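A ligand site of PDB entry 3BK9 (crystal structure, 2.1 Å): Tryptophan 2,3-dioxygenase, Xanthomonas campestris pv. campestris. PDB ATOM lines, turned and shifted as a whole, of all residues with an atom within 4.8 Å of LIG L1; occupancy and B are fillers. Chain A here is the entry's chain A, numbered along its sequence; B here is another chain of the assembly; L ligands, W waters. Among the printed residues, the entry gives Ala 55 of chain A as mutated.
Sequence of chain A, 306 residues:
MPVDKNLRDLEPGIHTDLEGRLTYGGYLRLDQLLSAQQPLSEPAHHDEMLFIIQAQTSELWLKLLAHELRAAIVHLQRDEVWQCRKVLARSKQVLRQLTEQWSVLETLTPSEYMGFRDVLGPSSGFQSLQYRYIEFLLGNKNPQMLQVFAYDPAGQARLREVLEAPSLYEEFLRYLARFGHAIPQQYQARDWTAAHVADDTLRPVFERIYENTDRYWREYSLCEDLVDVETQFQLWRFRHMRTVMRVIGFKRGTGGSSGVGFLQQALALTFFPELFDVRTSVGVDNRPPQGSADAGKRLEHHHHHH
A ring nitrogen (NE2) of His 240 is bound to an iron atom (FE1) of LIG L1 (2.3 Å).
The side-chain hydroxyl (OG) of Ser 124 sits at hydrogen-bond distance from an oxygen (O1) of LIG L1 (2.5 Å).
NH2 of Arg 132 lies within salt-bridge range of O3 of LIG L1, 2.6 Å away.
NH2 of Arg 8 of chain B is in salt-bridge range of O4 of LIG L1 (2.7 Å).
An oxygen (O2) of LIG L1 sits at hydrogen-bond distance from the backbone NH of Ser 257.
OG of Ser 257 sits at hydrogen-bond distance from O2 of LIG L1, 2.9 Å away.
The backbone NH of Gly 255 sits at hydrogen-bond distance from an oxygen (O1) of LIG L1 (3.1 Å).
N of Gly 256 is in hydrogen-bond range of O2 of LIG L1, 3.5 Å away.
An oxygen (O2) of LG2 L2 sits at hydrogen-bond distance from the backbone NH (N) of Thr 254, 3.1 Å away.
The side-chain hydroxyl of Thr 254 lies within hydrogen-bond range of a nitrogen (N1) of LG2 L2 (2.8 Å).
O1 of LG2 L2 lies within hydrogen-bond range of OH of Tyr 113 (2.7 Å).
N1 of LG2 L2 is in hydrogen-bond range of O1 of LIG L1, 3.2 Å away.
The side-chain hydroxyl (OG) of Ser 124 lies close to the backbone NH (N) of Phe 126.
The guanidinium group (NH2) of Arg 8 of chain B lies within hydrogen-bond range of the backbone carbonyl oxygen (O) of Phe 262 (3.3 Å).
N of Gly 259 is in hydrogen-bond range of OG of Ser 257 (2.8 Å).
The backbone NH (N) of Tyr 131 sits at hydrogen-bond distance from the side-chain hydroxyl (OG) of Ser 128 (3.1 Å).
O of Gln 54 sits at hydrogen-bond distance from OG of Ser 58 (3.0 Å).
Merely in contact with LIG L1: Phe 51 (3.7 Å), Gln 54 (3.6 Å), Ser 58 (3.7 Å), Trp 102 (3.6 Å), Leu 105 (3.9 Å), Gly 125 (3.4 Å), Phe 126 (3.5 Å), Tyr 131 (3.3 Å), Trp 236 (3.98 Å), Thr 243 (3.9 Å), Val 244 (3.3 Å), Val 247 (3.8 Å), Ile 248 (3.7 Å), Gly 253 (3.5 Å), Thr 254 (3.7 Å), Gly 259 (3.7 Å), Leu 263 (3.8 Å), Ala 266 (3.99 Å) and Tyr 24 of chain B (3.2 Å).
Of the 31 residues printed, 26 come within 4 Å of LIG L1.
Water W3 bridges the backbone NH of Gly 125 and a nitrogen (N1) of LG2 L2.
Water W1 bridges O4 of LIG L1 (2.8 Å) and NH1 of Arg 132 (3.0 Å).
Water W2 lies within hydrogen-bond range of a nitrogen (N2) of LG2 L2 (2.9 Å) and the backbone carbonyl oxygen of Phe 51 (3.5 Å).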
ATOM      1  N   PHE A  51       4.330 -11.566 -27.484  1.00  0.00           N
ATOM      2  CA  PHE A  51       4.375 -12.845 -26.885  1.00  0.00           C
ATOM      3  C   PHE A  51       2.987 -13.321 -26.616  1.00  0.00           C
ATOM      4  O   PHE A  51       2.672 -14.384 -26.974  1.00  0.00           O
ATOM      5  CB  PHE A  51       5.132 -12.672 -25.608  1.00  0.00           C
ATOM      6  CG  PHE A  51       5.755 -13.876 -25.139  1.00  0.00           C
ATOM      7  CD1 PHE A  51       6.830 -14.428 -25.843  1.00  0.00           C
ATOM      8  CD2 PHE A  51       5.251 -14.517 -24.004  1.00  0.00           C
ATOM      9  CE1 PHE A  51       7.432 -15.599 -25.430  1.00  0.00           C
ATOM     10  CE2 PHE A  51       5.864 -15.659 -23.578  1.00  0.00           C
ATOM     11  CZ  PHE A  51       6.961 -16.206 -24.341  1.00  0.00           C
ATOM     12  N   GLN A  54       0.732 -13.911 -29.999  1.00  0.00           N
ATOM     13  CA  GLN A  54       1.233 -14.940 -30.783  1.00  0.00           C
ATOM     14  C   GLN A  54       0.745 -16.263 -30.272  1.00  0.00           C
ATOM     15  O   GLN A  54       0.301 -17.088 -31.062  1.00  0.00           O
ATOM     16  CB  GLN A  54       2.746 -14.892 -30.658  1.00  0.00           C
ATOM     17  CG  GLN A  54       3.475 -15.982 -31.329  1.00  0.00           C
ATOM     18  CD  GLN A  54       3.733 -15.674 -32.817  1.00  0.00           C
ATOM     19  OE1 GLN A  54       3.771 -14.513 -33.194  1.00  0.00           O
ATOM     20  NE2 GLN A  54       3.953 -16.706 -33.652  1.00  0.00           N
ATOM     21  N   ALA A  55       0.874 -16.476 -28.958  1.00  0.00           N
ATOM     22  CA  ALA A  55       0.342 -17.678 -28.293  1.00  0.00           C
ATOM     23  C   ALA A  55      -1.168 -17.809 -28.316  1.00  0.00           C
ATOM     24  O   ALA A  55      -1.705 -18.893 -28.536  1.00  0.00           O
ATOM     25  CB  ALA A  55       0.909 -17.751 -26.792  1.00  0.00           C
ATOM     26  N   SER A  58      -2.438 -18.666 -31.897  1.00  0.00           N
ATOM     27  CA  SER A  58      -2.235 -20.106 -32.048  1.00  0.00           C
ATOM     28  C   SER A  58      -3.312 -20.989 -31.352  1.00  0.00           C
ATOM     29  O   SER A  58      -3.756 -21.935 -31.926  1.00  0.00           O
ATOM     30  CB  SER A  58      -0.819 -20.537 -31.544  1.00  0.00           C
ATOM     31  OG  SER A  58       0.176 -19.870 -32.277  1.00  0.00           O
ATOM     32  N   TRP A 102       5.238 -18.237 -37.207  1.00  0.00           N
ATOM     33  CA  TRP A 102       6.575 -18.108 -36.594  1.00  0.00           C
ATOM     34  C   TRP A 102       7.369 -16.976 -37.111  1.00  0.00           C
ATOM     35  O   TRP A 102       8.284 -16.529 -36.448  1.00  0.00           O
ATOM     36  CB  TRP A 102       7.393 -19.362 -36.715  1.00  0.00           C
ATOM     37  CG  TRP A 102       6.668 -20.495 -35.971  1.00  0.00           C
ATOM     38  CD1 TRP A 102       5.999 -21.512 -36.485  1.00  0.00           C
ATOM     39  CD2 TRP A 102       6.535 -20.582 -34.612  1.00  0.00           C
ATOM     40  NE1 TRP A 102       5.455 -22.294 -35.506  1.00  0.00           N
ATOM     41  CE2 TRP A 102       5.737 -21.702 -34.331  1.00  0.00           C
ATOM     42  CE3 TRP A 102       7.040 -19.831 -33.550  1.00  0.00           C
ATOM     43  CZ2 TRP A 102       5.463 -22.093 -33.043  1.00  0.00           C
ATOM     44  CZ3 TRP A 102       6.717 -20.239 -32.279  1.00  0.00           C
ATOM     45  CH2 TRP A 102       5.957 -21.326 -32.052  1.00  0.00           C
ATOM     46  N   LEU A 105       7.495 -13.918 -34.663  1.00  0.00           N
ATOM     47  CA  LEU A 105       8.219 -14.120 -33.446  1.00  0.00           C
ATOM     48  C   LEU A 105       9.717 -14.187 -33.769  1.00  0.00           C
ATOM     49  O   LEU A 105      10.516 -13.941 -32.914  1.00  0.00           O
ATOM     50  CB  LEU A 105       7.798 -15.439 -32.806  1.00  0.00           C
ATOM     51  CG  LEU A 105       7.728 -15.478 -31.306  1.00  0.00           C
ATOM     52  CD1 LEU A 105       7.275 -14.171 -30.821  1.00  0.00           C
ATOM     53  CD2 LEU A 105       6.808 -16.589 -30.816  1.00  0.00           C
ATOM     54  N   LEU A 108      11.721 -11.237 -32.453  1.00  0.00           N
ATOM     55  CA  LEU A 108      12.047 -11.221 -31.030  1.00  0.00           C
ATOM     56  C   LEU A 108      13.519 -11.747 -30.823  1.00  0.00           C
ATOM     57  O   LEU A 108      13.822 -12.900 -31.119  1.00  0.00           O
ATOM     58  CB  LEU A 108      11.078 -12.016 -30.183  1.00  0.00           C
ATOM     59  CG  LEU A 108      11.165 -11.941 -28.626  1.00  0.00           C
ATOM     60  CD1 LEU A 108      10.692 -10.672 -28.051  1.00  0.00           C
ATOM     61  CD2 LEU A 108      10.458 -13.141 -27.966  1.00  0.00           C
ATOM     62  N   TYR A 113      13.738 -10.681 -25.016  1.00  0.00           N
ATOM     63  CA  TYR A 113      13.119 -11.725 -24.243  1.00  0.00           C
ATOM     64  C   TYR A 113      13.487 -11.751 -22.760  1.00  0.00           C
ATOM     65  O   TYR A 113      12.579 -11.884 -21.939  1.00  0.00           O
ATOM     66  CB  TYR A 113      13.277 -13.074 -24.889  1.00  0.00           C
ATOM     67  CG  TYR A 113      12.323 -14.096 -24.353  1.00  0.00           C
ATOM     68  CD1 TYR A 113      12.751 -15.406 -24.126  1.00  0.00           C
ATOM     69  CD2 TYR A 113      10.987 -13.734 -24.016  1.00  0.00           C
ATOM     70  CE1 TYR A 113      11.886 -16.354 -23.716  1.00  0.00           C
ATOM     71  CE2 TYR A 113      10.113 -14.667 -23.553  1.00  0.00           C
ATOM     72  CZ  TYR A 113      10.584 -16.024 -23.446  1.00  0.00           C
ATOM     73  OH  TYR A 113       9.779 -17.012 -23.013  1.00  0.00           O
ATOM     74  N   SER A 124       4.293 -22.613 -19.718  1.00  0.00           N
ATOM     75  CA  SER A 124       4.878 -23.208 -20.916  1.00  0.00           C
ATOM     76  C   SER A 124       3.744 -23.728 -21.806  1.00  0.00           C
ATOM     77  O   SER A 124       2.765 -24.167 -21.264  1.00  0.00           O
ATOM     78  CB  SER A 124       5.796 -24.411 -20.545  1.00  0.00           C
ATOM     79  OG  SER A 124       6.281 -25.024 -21.710  1.00  0.00           O
ATOM     80  N   GLY A 125       3.912 -23.724 -23.163  1.00  0.00           N
ATOM     81  CA  GLY A 125       2.966 -24.407 -24.055  1.00  0.00           C
ATOM     82  C   GLY A 125       2.832 -25.898 -23.885  1.00  0.00           C
ATOM     83  O   GLY A 125       1.825 -26.538 -24.365  1.00  0.00           O
ATOM     84  N   PHE A 126       3.865 -26.510 -23.259  1.00  0.00           N
ATOM     85  CA  PHE A 126       3.760 -27.872 -22.827  1.00  0.00           C
ATOM     86  C   PHE A 126       2.504 -28.159 -22.011  1.00  0.00           C
ATOM     87  O   PHE A 126       1.898 -29.214 -22.113  1.00  0.00           O
ATOM     88  CB  PHE A 126       5.167 -28.311 -22.134  1.00  0.00           C
ATOM     89  CG  PHE A 126       5.165 -29.701 -21.641  1.00  0.00           C
ATOM     90  CD1 PHE A 126       5.536 -30.739 -22.473  1.00  0.00           C
ATOM     91  CD2 PHE A 126       4.726 -29.982 -20.326  1.00  0.00           C
ATOM     92  CE1 PHE A 126       5.456 -32.056 -21.997  1.00  0.00           C
ATOM     93  CE2 PHE A 126       4.612 -31.283 -19.875  1.00  0.00           C
ATOM     94  CZ  PHE A 126       5.019 -32.311 -20.709  1.00  0.00           C
ATOM     95  N   SER A 128      -0.364 -26.668 -22.738  1.00  0.00           N
ATOM     96  CA  SER A 128      -1.542 -26.479 -23.621  1.00  0.00           C
ATOM     97  C   SER A 128      -2.452 -27.683 -23.677  1.00  0.00           C
ATOM     98  O   SER A 128      -2.098 -28.669 -24.238  1.00  0.00           O
ATOM     99  CB  SER A 128      -1.119 -26.091 -25.029  1.00  0.00           C
ATOM    100  OG  SER A 128      -2.291 -25.964 -25.799  1.00  0.00           O
ATOM    101  N   TYR A 131      -3.396 -28.288 -27.466  1.00  0.00           N
ATOM    102  CA  TYR A 131      -2.388 -28.885 -28.278  1.00  0.00           C
ATOM    103  C   TYR A 131      -2.302 -30.427 -28.098  1.00  0.00           C
ATOM    104  O   TYR A 131      -2.108 -31.151 -29.106  1.00  0.00           O
ATOM    105  CB  TYR A 131      -1.045 -28.144 -27.972  1.00  0.00           C
ATOM    106  CG  TYR A 131       0.095 -28.780 -28.640  1.00  0.00           C
ATOM    107  CD1 TYR A 131       0.434 -28.420 -29.940  1.00  0.00           C
ATOM    108  CD2 TYR A 131       0.853 -29.789 -27.987  1.00  0.00           C
ATOM    109  CE1 TYR A 131       1.409 -29.073 -30.568  1.00  0.00           C
ATOM    110  CE2 TYR A 131       1.909 -30.403 -28.618  1.00  0.00           C
ATOM    111  CZ  TYR A 131       2.186 -30.076 -29.903  1.00  0.00           C
ATOM    112  OH  TYR A 131       3.230 -30.683 -30.616  1.00  0.00           O
ATOM    113  N   ARG A 132      -2.372 -30.861 -26.814  1.00  0.00           N
ATOM    114  CA  ARG A 132      -2.318 -32.265 -26.318  1.00  0.00           C
ATOM    115  C   ARG A 132      -3.515 -33.070 -26.771  1.00  0.00           C
ATOM    116  O   ARG A 132      -3.434 -34.191 -27.039  1.00  0.00           O
ATOM    117  CB  ARG A 132      -2.227 -32.290 -24.751  1.00  0.00           C
ATOM    118  CG  ARG A 132      -1.551 -33.604 -24.106  1.00  0.00           C
ATOM    119  CD  ARG A 132      -0.257 -34.086 -24.824  1.00  0.00           C
ATOM    120  NE  ARG A 132       0.739 -33.019 -24.795  1.00  0.00           N
ATOM    121  CZ  ARG A 132       1.871 -32.933 -25.497  1.00  0.00           C
ATOM    122  NH1 ARG A 132       2.205 -33.896 -26.343  1.00  0.00           N
ATOM    123  NH2 ARG A 132       2.647 -31.831 -25.353  1.00  0.00           N
ATOM    124  N   TRP A 236       5.465 -27.362 -38.441  1.00  0.00           N
ATOM    125  CA  TRP A 236       5.092 -26.574 -37.248  1.00  0.00           C
ATOM    126  C   TRP A 236       6.113 -26.796 -36.122  1.00  0.00           C
ATOM    127  O   TRP A 236       6.627 -25.848 -35.576  1.00  0.00           O
ATOM    128  CB  TRP A 236       3.635 -26.826 -36.765  1.00  0.00           C
ATOM    129  CG  TRP A 236       3.385 -25.966 -35.481  1.00  0.00           C
ATOM    130  CD1 TRP A 236       2.915 -24.704 -35.459  1.00  0.00           C
ATOM    131  CD2 TRP A 236       3.696 -26.316 -34.083  1.00  0.00           C
ATOM    132  NE1 TRP A 236       2.842 -24.255 -34.175  1.00  0.00           N
ATOM    133  CE2 TRP A 236       3.353 -25.188 -33.310  1.00  0.00           C
ATOM    134  CE3 TRP A 236       4.251 -27.449 -33.430  1.00  0.00           C
ATOM    135  CZ2 TRP A 236       3.482 -25.173 -31.872  1.00  0.00           C
ATOM    136  CZ3 TRP A 236       4.477 -27.391 -32.008  1.00  0.00           C
ATOM    137  CH2 TRP A 236       4.086 -26.280 -31.252  1.00  0.00           C
ATOM    138  N   HIS A 240       8.868 -23.926 -34.613  1.00  0.00           N
ATOM    139  CA  HIS A 240       8.866 -23.708 -33.189  1.00  0.00           C
ATOM    140  C   HIS A 240      10.247 -23.948 -32.538  1.00  0.00           C
ATOM    141  O   HIS A 240      10.822 -23.043 -31.847  1.00  0.00           O
ATOM    142  CB  HIS A 240       7.799 -24.640 -32.539  1.00  0.00           C
ATOM    143  CG  HIS A 240       7.806 -24.629 -31.021  1.00  0.00           C
ATOM    144  ND1 HIS A 240       8.032 -25.751 -30.260  1.00  0.00           N
ATOM    145  CD2 HIS A 240       7.631 -23.614 -30.154  1.00  0.00           C
ATOM    146  CE1 HIS A 240       7.969 -25.441 -28.991  1.00  0.00           C
ATOM    147  NE2 HIS A 240       7.764 -24.135 -28.901  1.00  0.00           N
ATOM    148  N   THR A 243      12.801 -21.398 -33.585  1.00  0.00           N
ATOM    149  CA  THR A 243      12.535 -20.168 -32.841  1.00  0.00           C
ATOM    150  C   THR A 243      13.087 -20.256 -31.371  1.00  0.00           C
ATOM    151  O   THR A 243      13.762 -19.319 -30.862  1.00  0.00           O
ATOM    152  CB  THR A 243      11.037 -19.814 -32.949  1.00  0.00           C
ATOM    153  OG1 THR A 243      10.646 -19.883 -34.344  1.00  0.00           O
ATOM    154  CG2 THR A 243      10.744 -18.375 -32.360  1.00  0.00           C
ATOM    155  N   VAL A 244      12.818 -21.370 -30.694  1.00  0.00           N
ATOM    156  CA  VAL A 244      13.523 -21.705 -29.476  1.00  0.00           C
ATOM    157  C   VAL A 244      15.042 -21.535 -29.552  1.00  0.00           C
ATOM    158  O   VAL A 244      15.582 -20.827 -28.725  1.00  0.00           O
ATOM    159  CB  VAL A 244      13.068 -23.098 -28.893  1.00  0.00           C
ATOM    160  CG1 VAL A 244      13.727 -23.307 -27.620  1.00  0.00           C
ATOM    161  CG2 VAL A 244      11.565 -23.118 -28.727  1.00  0.00           C
ATOM    162  N   VAL A 247      15.846 -17.822 -29.630  1.00  0.00           N
ATOM    163  CA  VAL A 247      15.410 -16.920 -28.598  1.00  0.00           C
ATOM    164  C   VAL A 247      16.087 -17.306 -27.280  1.00  0.00           C
ATOM    165  O   VAL A 247      16.613 -16.461 -26.609  1.00  0.00           O
ATOM    166  CB  VAL A 247      13.869 -16.912 -28.498  1.00  0.00           C
ATOM    167  CG1 VAL A 247      13.352 -16.106 -27.318  1.00  0.00           C
ATOM    168  CG2 VAL A 247      13.204 -16.388 -29.847  1.00  0.00           C
ATOM    169  N   ILE A 248      16.074 -18.584 -26.900  1.00  0.00           N
ATOM    170  CA  ILE A 248      16.717 -19.037 -25.652  1.00  0.00           C
ATOM    171  C   ILE A 248      17.963 -19.960 -25.833  1.00  0.00           C
ATOM    172  O   ILE A 248      18.593 -20.333 -24.876  1.00  0.00           O
ATOM    173  CB  ILE A 248      15.708 -19.726 -24.658  1.00  0.00           C
ATOM    174  CG1 ILE A 248      15.137 -21.048 -25.219  1.00  0.00           C
ATOM    175  CG2 ILE A 248      14.592 -18.809 -24.366  1.00  0.00           C
ATOM    176  CD1 ILE A 248      14.329 -21.953 -24.113  1.00  0.00           C
ATOM    177  N   GLY A 253      13.859 -25.076 -20.545  1.00  0.00           N
ATOM    178  CA  GLY A 253      12.602 -24.352 -20.710  1.00  0.00           C
ATOM    179  C   GLY A 253      11.981 -23.907 -19.409  1.00  0.00           C
ATOM    180  O   GLY A 253      12.353 -24.391 -18.333  1.00  0.00           O
ATOM    181  N   THR A 254      11.014 -22.985 -19.505  1.00  0.00           N
ATOM    182  CA  THR A 254      10.239 -22.480 -18.377  1.00  0.00           C
ATOM    183  C   THR A 254       9.498 -23.598 -17.659  1.00  0.00           C
ATOM    184  O   THR A 254       9.342 -23.534 -16.465  1.00  0.00           O
ATOM    185  CB  THR A 254       9.264 -21.355 -18.747  1.00  0.00           C
ATOM    186  OG1 THR A 254       8.482 -21.733 -19.893  1.00  0.00           O
ATOM    187  CG2 THR A 254      10.031 -20.037 -19.026  1.00  0.00           C
ATOM    188  N   GLY A 255       9.009 -24.586 -18.423  1.00  0.00           N
ATOM    189  CA  GLY A 255       8.269 -25.737 -17.952  1.00  0.00           C
ATOM    190  C   GLY A 255       9.077 -26.923 -17.415  1.00  0.00           C
ATOM    191  O   GLY A 255       8.512 -27.932 -17.013  1.00  0.00           O
ATOM    192  N   GLY A 256      10.400 -26.781 -17.456  1.00  0.00           N
ATOM    193  CA  GLY A 256      11.334 -27.630 -16.692  1.00  0.00           C
ATOM    194  C   GLY A 256      12.080 -28.602 -17.581  1.00  0.00           C
ATOM    195  O   GLY A 256      12.991 -29.270 -17.110  1.00  0.00           O
ATOM    196  N   SER A 257      11.770 -28.601 -18.888  1.00  0.00           N
ATOM    197  CA  SER A 257      12.334 -29.583 -19.773  1.00  0.00           C
ATOM    198  C   SER A 257      13.665 -29.065 -20.195  1.00  0.00           C
ATOM    199  O   SER A 257      13.979 -27.902 -19.979  1.00  0.00           O
ATOM    200  CB  SER A 257      11.462 -29.786 -20.998  1.00  0.00           C
ATOM    201  OG  SER A 257      11.867 -28.901 -22.051  1.00  0.00           O
ATOM    202  N   GLY A 259      14.402 -28.430 -23.054  1.00  0.00           N
ATOM    203  CA  GLY A 259      14.141 -27.469 -24.099  1.00  0.00           C
ATOM    204  C   GLY A 259      14.386 -28.051 -25.475  1.00  0.00           C
ATOM    205  O   GLY A 259      13.637 -28.906 -25.903  1.00  0.00           O
ATOM    206  N   PHE A 262      14.466 -31.801 -25.790  1.00  0.00           N
ATOM    207  CA  PHE A 262      13.071 -32.324 -25.566  1.00  0.00           C
ATOM    208  C   PHE A 262      12.136 -32.136 -26.774  1.00  0.00           C
ATOM    209  O   PHE A 262      11.324 -33.045 -27.112  1.00  0.00           O
ATOM    210  CB  PHE A 262      12.446 -31.732 -24.308  1.00  0.00           C
ATOM    211  CG  PHE A 262      11.128 -32.370 -23.854  1.00  0.00           C
ATOM    212  CD1 PHE A 262      10.004 -31.571 -23.739  1.00  0.00           C
ATOM    213  CD2 PHE A 262      11.061 -33.715 -23.413  1.00  0.00           C
ATOM    214  CE1 PHE A 262       8.800 -32.084 -23.379  1.00  0.00           C
ATOM    215  CE2 PHE A 262       9.879 -34.224 -22.919  1.00  0.00           C
ATOM    216  CZ  PHE A 262       8.720 -33.401 -22.903  1.00  0.00           C
ATOM    217  N   LEU A 263      12.265 -30.988 -27.440  1.00  0.00           N
ATOM    218  CA  LEU A 263      11.411 -30.720 -28.671  1.00  0.00           C
ATOM    219  C   LEU A 263      11.878 -31.546 -29.830  1.00  0.00           C
ATOM    220  O   LEU A 263      11.042 -32.034 -30.639  1.00  0.00           O
ATOM    221  CB  LEU A 263      11.483 -29.244 -29.145  1.00  0.00           C
ATOM    222  CG  LEU A 263      10.927 -28.332 -28.036  1.00  0.00           C
ATOM    223  CD1 LEU A 263      11.451 -26.887 -28.220  1.00  0.00           C
ATOM    224  CD2 LEU A 263       9.469 -28.508 -27.798  1.00  0.00           C
ATOM    225  N   ALA A 266      10.142 -35.170 -30.019  1.00  0.00           N
ATOM    226  CA  ALA A 266       8.844 -35.202 -30.757  1.00  0.00           C
ATOM    227  C   ALA A 266       8.999 -35.177 -32.283  1.00  0.00           C
ATOM    228  O   ALA A 266       8.253 -35.789 -32.997  1.00  0.00           O
ATOM    229  CB  ALA A 266       7.951 -34.001 -30.275  1.00  0.00           C
ATOM    230  N   ARG B   8       7.632 -40.443 -26.719  1.00  0.00           N
ATOM    231  CA  ARG B   8       8.584 -39.604 -25.973  1.00  0.00           C
ATOM    232  C   ARG B   8       8.309 -39.699 -24.451  1.00  0.00           C
ATOM    233  O   ARG B   8       7.170 -39.546 -23.945  1.00  0.00           O
ATOM    234  CB  ARG B   8       8.524 -38.197 -26.522  1.00  0.00           C
ATOM    235  CG  ARG B   8       9.433 -37.079 -25.978  1.00  0.00           C
ATOM    236  CD  ARG B   8       8.497 -36.180 -25.346  1.00  0.00           C
ATOM    237  NE  ARG B   8       8.540 -34.974 -26.044  1.00  0.00           N
ATOM    238  CZ  ARG B   8       7.655 -33.980 -26.027  1.00  0.00           C
ATOM    239  NH1 ARG B   8       6.466 -33.963 -25.382  1.00  0.00           N
ATOM    240  NH2 ARG B   8       8.045 -32.969 -26.714  1.00  0.00           N
ATOM    241  N   TYR B  24       0.056 -21.497 -17.687  1.00  0.00           N
ATOM    242  CA  TYR B  24      -0.025 -21.080 -19.116  1.00  0.00           C
ATOM    243  C   TYR B  24      -1.413 -20.471 -19.454  1.00  0.00           C
ATOM    244  O   TYR B  24      -1.533 -19.374 -19.958  1.00  0.00           O
ATOM    245  CB  TYR B  24       0.242 -22.319 -19.941  1.00  0.00           C
ATOM    246  CG  TYR B  24       0.003 -22.207 -21.404  1.00  0.00           C
ATOM    247  CD1 TYR B  24      -1.187 -22.757 -22.022  1.00  0.00           C
ATOM    248  CD2 TYR B  24       0.972 -21.624 -22.223  1.00  0.00           C
ATOM    249  CE1 TYR B  24      -1.342 -22.709 -23.441  1.00  0.00           C
ATOM    250  CE2 TYR B  24       0.797 -21.602 -23.638  1.00  0.00           C
ATOM    251  CZ  TYR B  24      -0.397 -22.104 -24.220  1.00  0.00           C
ATOM    252  OH  TYR B  24      -0.483 -22.028 -25.624  1.00  0.00           O
HETATM  253  C1  LIG L   1       7.217 -26.398 -25.657  1.00  0.00           C
HETATM  254  C2  LIG L   1      10.135 -22.643 -25.807  1.00  0.00           C
HETATM  255  C3  LIG L   1       6.675 -20.126 -28.135  1.00  0.00           C
HETATM  256  C4  LIG L   1       3.699 -23.911 -28.078  1.00  0.00           C
HETATM  257  C5  LIG L   1       8.316 -25.593 -25.401  1.00  0.00           C
HETATM  258  C6  LIG L   1       9.450 -25.916 -24.618  1.00  0.00           C
HETATM  259  C7  LIG L   1      10.302 -24.870 -24.644  1.00  0.00           C
HETATM  260  C8  LIG L   1       9.660 -23.885 -25.460  1.00  0.00           C
HETATM  261  C9  LIG L   1      11.743 -24.611 -24.085  1.00  0.00           C
HETATM  262  C10 LIG L   1       9.490 -27.367 -23.966  1.00  0.00           C
HETATM  263  C11 LIG L   1       8.556 -27.336 -22.708  1.00  0.00           C
HETATM  264  C12 LIG L   1       9.238 -26.442 -21.629  1.00  0.00           C
HETATM  265  O1  LIG L   1       8.794 -25.280 -21.426  1.00  0.00           O
HETATM  266  O2  LIG L   1      10.230 -26.848 -20.936  1.00  0.00           O
HETATM  267  C13 LIG L   1       9.453 -21.638 -26.397  1.00  0.00           C
HETATM  268  C14 LIG L   1       9.940 -20.285 -26.625  1.00  0.00           C
HETATM  269  C15 LIG L   1       8.979 -19.610 -27.312  1.00  0.00           C
HETATM  270  C16 LIG L   1       7.853 -20.480 -27.536  1.00  0.00           C
HETATM  271  C17 LIG L   1      11.307 -19.744 -26.144  1.00  0.00           C
HETATM  272  C18 LIG L   1       8.995 -18.132 -27.703  1.00  0.00           C
HETATM  273  C19 LIG L   1       9.866 -17.663 -28.576  1.00  0.00           C
HETATM  274  C20 LIG L   1       5.539 -20.874 -28.305  1.00  0.00           C
HETATM  275  C21 LIG L   1       4.290 -20.472 -28.947  1.00  0.00           C
HETATM  276  C22 LIG L   1       3.473 -21.522 -28.922  1.00  0.00           C
HETATM  277  C23 LIG L   1       4.176 -22.628 -28.298  1.00  0.00           C
HETATM  278  C24 LIG L   1       3.987 -19.089 -29.494  1.00  0.00           C
HETATM  279  C25 LIG L   1       2.029 -21.683 -29.429  1.00  0.00           C
HETATM  280  C26 LIG L   1       1.120 -22.063 -28.440  1.00  0.00           C
HETATM  281  C27 LIG L   1       4.430 -24.894 -27.484  1.00  0.00           C
HETATM  282  C28 LIG L   1       3.873 -26.165 -27.246  1.00  0.00           C
HETATM  283  C29 LIG L   1       4.973 -26.937 -26.558  1.00  0.00           C
HETATM  284  C30 LIG L   1       6.070 -26.018 -26.313  1.00  0.00           C
HETATM  285  C31 LIG L   1       2.523 -26.814 -27.635  1.00  0.00           C
HETATM  286  C32 LIG L   1       4.772 -28.393 -26.195  1.00  0.00           C
HETATM  287  C33 LIG L   1       5.565 -29.107 -27.308  1.00  0.00           C
HETATM  288  C34 LIG L   1       5.648 -30.608 -27.017  1.00  0.00           C
HETATM  289  O3  LIG L   1       5.035 -31.126 -26.000  1.00  0.00           O
HETATM  290  O4  LIG L   1       6.306 -31.290 -27.849  1.00  0.00           O
HETATM  291  N1  LIG L   1       8.489 -24.359 -25.934  1.00  0.00           N
HETATM  292  N2  LIG L   1       8.191 -21.771 -27.033  1.00  0.00           N
HETATM  293  N3  LIG L   1       5.426 -22.241 -27.938  1.00  0.00           N
HETATM  294  N4  LIG L   1       5.713 -24.764 -26.919  1.00  0.00           N
HETATM  295 FE1  LIG L   1       6.963 -23.233 -26.945  1.00  0.00          FE
HETATM  296  N1  LG2 L   2       8.379 -22.331 -22.647  1.00  0.00           N
HETATM  297  C1  LG2 L   2       8.818 -21.021 -23.151  1.00  0.00           C
HETATM  298  C2  LG2 L   2      10.208 -20.702 -22.637  1.00  0.00           C
HETATM  299  O1  LG2 L   2      10.585 -19.562 -22.569  1.00  0.00           O
HETATM  300  C3  LG2 L   2       7.946 -19.891 -22.630  1.00  0.00           C
HETATM  301  C4  LG2 L   2       6.795 -19.467 -23.492  1.00  0.00           C
HETATM  302  C5  LG2 L   2       6.799 -19.220 -24.784  1.00  0.00           C
HETATM  303  C6  LG2 L   2       5.470 -19.138 -22.984  1.00  0.00           C
HETATM  304  N2  LG2 L   2       5.468 -18.740 -25.193  1.00  0.00           N
HETATM  305  C7  LG2 L   2       4.682 -18.707 -24.068  1.00  0.00           C
HETATM  306  C8  LG2 L   2       4.893 -19.145 -21.690  1.00  0.00           C
HETATM  307  C9  LG2 L   2       3.354 -18.298 -23.904  1.00  0.00           C
HETATM  308  C10 LG2 L   2       3.601 -18.770 -21.532  1.00  0.00           C
HETATM  309  C11 LG2 L   2       2.842 -18.336 -22.622  1.00  0.00           C
HETATM  310  O2  LG2 L   2      10.953 -21.560 -22.203  1.00  0.00           O
HETATM  311  O   HOH W   1       4.479 -33.425 -28.318  1.00  0.00           O
HETATM  312  O   HOH W   2       5.137 -16.812 -27.389  1.00  0.00           O
HETATM  313  O   HOH W   3       6.006 -22.464 -24.448  1.00  0.00           O
